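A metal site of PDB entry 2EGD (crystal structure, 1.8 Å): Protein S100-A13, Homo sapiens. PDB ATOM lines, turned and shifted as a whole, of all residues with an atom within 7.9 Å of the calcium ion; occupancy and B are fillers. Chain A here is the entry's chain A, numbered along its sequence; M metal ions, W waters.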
ATOM      1  N   SER A  32      24.250 -27.201  -4.205  1.00  0.00           N
ATOM      2  CA  SER A  32      23.136 -26.449  -3.621  1.00  0.00           C
ATOM      3  C   SER A  32      22.639 -27.045  -2.312  1.00  0.00           C
ATOM      4  O   SER A  32      22.787 -28.248  -2.067  1.00  0.00           O
ATOM      5  CB  SER A  32      22.010 -26.204  -4.619  1.00  0.00           C
ATOM      6  OG  SER A  32      21.291 -27.380  -4.823  1.00  0.00           O
ATOM      7  N   LEU A  33      22.088 -26.173  -1.470  1.00  0.00           N
ATOM      8  CA  LEU A  33      21.494 -26.548  -0.184  1.00  0.00           C
ATOM      9  C   LEU A  33      19.999 -26.854  -0.365  1.00  0.00           C
ATOM     10  O   LEU A  33      19.240 -25.981  -0.808  1.00  0.00           O
ATOM     11  CB  LEU A  33      21.622 -25.364   0.805  1.00  0.00           C
ATOM     12  CG  LEU A  33      23.050 -25.023   1.191  1.00  0.00           C
ATOM     13  CD1 LEU A  33      23.010 -23.691   1.946  1.00  0.00           C
ATOM     14  CD2 LEU A  33      23.736 -26.055   2.023  1.00  0.00           C
ATOM     15  N   MET A  60      14.145 -20.182   4.462  1.00  0.00           N
ATOM     16  CA  MET A  60      14.533 -20.873   3.208  1.00  0.00           C
ATOM     17  C   MET A  60      13.775 -20.257   1.997  1.00  0.00           C
ATOM     18  O   MET A  60      14.379 -19.853   0.980  1.00  0.00           O
ATOM     19  CB  MET A  60      14.210 -22.364   3.333  1.00  0.00           C
ATOM     20  CG  MET A  60      14.468 -23.204   2.060  1.00  0.00           C
ATOM     21  SD  MET A  60      16.247 -23.538   1.861  1.00  0.00           S
ATOM     22  CE  MET A  60      16.227 -24.498   0.361  1.00  0.00           C
ATOM     23  N   LYS A  61      12.479 -20.161   2.125  1.00  0.00           N
ATOM     24  CA  LYS A  61      11.606 -19.590   1.091  1.00  0.00           C
ATOM     25  C   LYS A  61      12.069 -18.177   0.749  1.00  0.00           C
ATOM     26  O   LYS A  61      12.248 -17.867  -0.376  1.00  0.00           O
ATOM     27  CB  LYS A  61      10.124 -19.638   1.508  1.00  0.00           C
ATOM     28  CG  LYS A  61       9.506 -21.070   1.510  1.00  0.00           C
ATOM     29  CD  LYS A  61       8.008 -21.093   1.904  1.00  0.00           C
ATOM     30  N   LEU A  63      15.075 -16.768   1.130  1.00  0.00           N
ATOM     31  CA  LEU A  63      16.384 -16.794   0.470  1.00  0.00           C
ATOM     32  C   LEU A  63      16.361 -17.428  -0.900  1.00  0.00           C
ATOM     33  O   LEU A  63      17.297 -17.241  -1.680  1.00  0.00           O
ATOM     34  CB  LEU A  63      17.397 -17.559   1.339  1.00  0.00           C
ATOM     35  CG  LEU A  63      17.752 -16.907   2.674  1.00  0.00           C
ATOM     36  CD1 LEU A  63      18.498 -17.873   3.567  1.00  0.00           C
ATOM     37  CD2 LEU A  63      18.623 -15.615   2.484  1.00  0.00           C
ATOM     38  N   ASP A  64      15.374 -18.270  -1.160  1.00  0.00           N
ATOM     39  CA  ASP A  64      15.296 -18.994  -2.419  1.00  0.00           C
ATOM     40  C   ASP A  64      14.689 -18.040  -3.471  1.00  0.00           C
ATOM     41  O   ASP A  64      13.506 -18.160  -3.824  1.00  0.00           O
ATOM     42  CB  ASP A  64      14.529 -20.314  -2.232  1.00  0.00           C
ATOM     43  CG  ASP A  64      14.276 -21.035  -3.558  1.00  0.00           C
ATOM     44  OD1 ASP A  64      15.090 -20.823  -4.515  1.00  0.00           O
ATOM     45  OD2 ASP A  64      13.297 -21.808  -3.660  1.00  0.00           O
ATOM     46  N   VAL A  65      15.506 -17.101  -3.972  1.00  0.00           N
ATOM     47  CA  VAL A  65      14.994 -15.997  -4.787  1.00  0.00           C
ATOM     48  C   VAL A  65      14.496 -16.345  -6.191  1.00  0.00           C
ATOM     49  O   VAL A  65      13.818 -15.543  -6.817  1.00  0.00           O
ATOM     50  CB  VAL A  65      16.016 -14.868  -4.908  1.00  0.00           C
ATOM     51  CG1 VAL A  65      16.306 -14.290  -3.517  1.00  0.00           C
ATOM     52  CG2 VAL A  65      17.309 -15.371  -5.551  1.00  0.00           C
ATOM     53  N   ASN A  66      14.863 -17.518  -6.688  1.00  0.00           N
ATOM     54  CA  ASN A  66      14.314 -18.019  -7.976  1.00  0.00           C
ATOM     55  C   ASN A  66      13.348 -19.192  -7.805  1.00  0.00           C
ATOM     56  O   ASN A  66      12.996 -19.830  -8.792  1.00  0.00           O
ATOM     57  CB  ASN A  66      15.438 -18.432  -8.888  1.00  0.00           C
ATOM     58  CG  ASN A  66      16.532 -19.109  -8.148  1.00  0.00           C
ATOM     59  OD1 ASN A  66      16.310 -20.106  -7.387  1.00  0.00           O
ATOM     60  ND2 ASN A  66      17.728 -18.557  -8.280  1.00  0.00           N
ATOM     61  N   GLN A  67      12.961 -19.486  -6.565  1.00  0.00           N
ATOM     62  CA  GLN A  67      11.817 -20.380  -6.329  1.00  0.00           C
ATOM     63  C   GLN A  67      12.039 -21.753  -6.951  1.00  0.00           C
ATOM     64  O   GLN A  67      11.158 -22.308  -7.606  1.00  0.00           O
ATOM     65  CB  GLN A  67      10.521 -19.717  -6.842  1.00  0.00           C
ATOM     66  CG  GLN A  67      10.350 -18.343  -6.223  1.00  0.00           C
ATOM     67  CD  GLN A  67       9.960 -17.257  -7.208  1.00  0.00           C
ATOM     68  OE1 GLN A  67       9.736 -17.505  -8.388  1.00  0.00           O
ATOM     69  NE2 GLN A  67       9.881 -16.040  -6.726  1.00  0.00           N
ATOM     70  N   ASP A  68      13.228 -22.314  -6.739  1.00  0.00           N
ATOM     71  CA  ASP A  68      13.557 -23.667  -7.184  1.00  0.00           C
ATOM     72  C   ASP A  68      13.800 -24.680  -6.045  1.00  0.00           C
ATOM     73  O   ASP A  68      14.157 -25.828  -6.299  1.00  0.00           O
ATOM     74  CB  ASP A  68      14.698 -23.668  -8.206  1.00  0.00           C
ATOM     75  CG  ASP A  68      16.035 -23.278  -7.593  1.00  0.00           C
ATOM     76  OD1 ASP A  68      16.078 -23.001  -6.390  1.00  0.00           O
ATOM     77  OD2 ASP A  68      17.025 -23.225  -8.334  1.00  0.00           O
ATOM     78  N   SER A  69      13.591 -24.231  -4.809  1.00  0.00           N
ATOM     79  CA  SER A  69      13.543 -25.058  -3.593  1.00  0.00           C
ATOM     80  C   SER A  69      14.930 -25.459  -3.113  1.00  0.00           C
ATOM     81  O   SER A  69      15.055 -26.357  -2.272  1.00  0.00           O
ATOM     82  CB  SER A  69      12.665 -26.321  -3.768  1.00  0.00           C
ATOM     83  OG  SER A  69      11.386 -25.976  -4.283  1.00  0.00           O
ATOM     84  N   GLU A  70      15.944 -24.775  -3.644  1.00  0.00           N
ATOM     85  CA  GLU A  70      17.349 -24.987  -3.277  1.00  0.00           C
ATOM     86  C   GLU A  70      18.060 -23.654  -3.119  1.00  0.00           C
ATOM     87  O   GLU A  70      17.694 -22.700  -3.762  1.00  0.00           O
ATOM     88  CB  GLU A  70      18.106 -25.804  -4.357  1.00  0.00           C
ATOM     89  CG  GLU A  70      17.490 -27.151  -4.680  1.00  0.00           C
ATOM     90  CD  GLU A  70      18.147 -28.350  -4.005  1.00  0.00           C
ATOM     91  OE1 GLU A  70      17.468 -29.365  -3.867  1.00  0.00           O
ATOM     92  OE2 GLU A  70      19.338 -28.303  -3.633  1.00  0.00           O
ATOM     93  N   LEU A  71      19.101 -23.608  -2.283  1.00  0.00           N
ATOM     94  CA  LEU A  71      19.916 -22.396  -2.231  1.00  0.00           C
ATOM     95  C   LEU A  71      21.247 -22.676  -2.952  1.00  0.00           C
ATOM     96  O   LEU A  71      22.030 -23.494  -2.471  1.00  0.00           O
ATOM     97  CB  LEU A  71      20.209 -21.987  -0.773  1.00  0.00           C
ATOM     98  CG  LEU A  71      18.940 -21.747   0.062  1.00  0.00           C
ATOM     99  CD1 LEU A  71      19.289 -21.092   1.370  1.00  0.00           C
ATOM    100  CD2 LEU A  71      17.916 -20.903  -0.746  1.00  0.00           C
ATOM    101  N   LYS A  72      21.491 -21.979  -4.083  1.00  0.00           N
ATOM    102  CA  LYS A  72      22.789 -22.024  -4.750  1.00  0.00           C
ATOM    103  C   LYS A  72      23.724 -21.088  -4.013  1.00  0.00           C
ATOM    104  O   LYS A  72      23.291 -20.374  -3.088  1.00  0.00           O
ATOM    105  CB  LYS A  72      22.687 -21.689  -6.251  1.00  0.00           C
ATOM    106  CG  LYS A  72      22.056 -22.875  -7.033  1.00  0.00           C
ATOM    107  CD  LYS A  72      22.121 -22.722  -8.514  1.00  0.00           C
ATOM    108  CE  LYS A  72      20.971 -23.488  -9.147  1.00  0.00           C
ATOM    109  NZ  LYS A  72      20.740 -23.134 -10.614  1.00  0.00           N
ATOM    110  N   PHE A  73      25.005 -21.102  -4.368  1.00  0.00           N
ATOM    111  CA  PHE A  73      25.984 -20.330  -3.585  1.00  0.00           C
ATOM    112  C   PHE A  73      25.588 -18.840  -3.583  1.00  0.00           C
ATOM    113  O   PHE A  73      25.721 -18.147  -2.562  1.00  0.00           O
ATOM    114  CB  PHE A  73      27.382 -20.437  -4.184  1.00  0.00           C
ATOM    115  CG  PHE A  73      28.383 -19.644  -3.446  1.00  0.00           C
ATOM    116  CD1 PHE A  73      28.874 -20.104  -2.224  1.00  0.00           C
ATOM    117  CD2 PHE A  73      28.775 -18.372  -3.914  1.00  0.00           C
ATOM    118  CE1 PHE A  73      29.774 -19.315  -1.481  1.00  0.00           C
ATOM    119  CE2 PHE A  73      29.684 -17.594  -3.188  1.00  0.00           C
ATOM    120  CZ  PHE A  73      30.187 -18.066  -1.969  1.00  0.00           C
ATOM    121  N   ASN A  74      25.099 -18.327  -4.699  1.00  0.00           N
ATOM    122  CA  ASN A  74      24.723 -16.899  -4.730  1.00  0.00           C
ATOM    123  C   ASN A  74      23.687 -16.542  -3.674  1.00  0.00           C
ATOM    124  O   ASN A  74      23.716 -15.443  -3.082  1.00  0.00           O
ATOM    125  CB  ASN A  74      24.353 -16.373  -6.150  1.00  0.00           C
ATOM    126  CG  ASN A  74      23.180 -17.139  -6.858  1.00  0.00           C
ATOM    127  OD1 ASN A  74      22.540 -18.059  -6.325  1.00  0.00           O
ATOM    128  ND2 ASN A  74      22.950 -16.759  -8.134  1.00  0.00           N
ATOM    129  N   GLU A  75      22.756 -17.471  -3.440  1.00  0.00           N
ATOM    130  CA  GLU A  75      21.655 -17.208  -2.484  1.00  0.00           C
ATOM    131  C   GLU A  75      22.163 -17.280  -1.048  1.00  0.00           C
ATOM    132  O   GLU A  75      21.750 -16.494  -0.185  1.00  0.00           O
ATOM    133  CB  GLU A  75      20.466 -18.149  -2.730  1.00  0.00           C
ATOM    134  CG  GLU A  75      19.712 -17.838  -4.084  1.00  0.00           C
ATOM    135  CD  GLU A  75      18.855 -18.969  -4.561  1.00  0.00           C
ATOM    136  OE1 GLU A  75      19.217 -20.181  -4.402  1.00  0.00           O
ATOM    137  OE2 GLU A  75      17.761 -18.666  -5.073  1.00  0.00           O
HETATM  138 CA    CA M   1      17.202 -21.149  -5.416  1.00  0.00          CA
HETATM  139  O   HOH W   1      18.870 -21.669  -6.925  1.00  0.00           O
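Five residues have an atom within 4 Å of the calcium ion: Asp 64, Asn 66, Asp 68, Glu 70 and Glu 75.
Water W1 is bound to the calcium ion.
The side-chain carboxylate (OD1) of Asp 64 binds the calcium ion (2.3 Å).
The calcium ion is bound by O of Glu 70 (2.3 Å).
The side-chain carboxylate (OD1) of Asp 68 binds the calcium ion, 2.4 Å away.
The calcium ion is bound by OD1 of Asn 66 (2.4 Å).
The calcium ion is bound by the side-chain carboxylate (OE1) of Glu 75, at 2.5 Å.
The side-chain carboxylate (OE2) of Glu 75 is bound to the calcium ion, at 2.6 Å.
The calcium ion has seven donor atoms within binding distance.
The side-chain carboxylate of Glu 75 sits close to the backbone NH of Val 65 (3.0 Å).
The side-chain hydroxyl of Ser 32 lies within hydrogen-bond range of the side-chain carboxylate of Glu 70.
OD2 of Asp 64 lies within hydrogen-bond range of N of Ser 69 (2.7 Å).
OD1 of Asp 64 sits close to N of Gln 67 (3.2 Å).
The side-chain carboxylate (OE1) of Glu 75 lies close to the backbone NH (N) of Lys 72 (2.9 Å).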
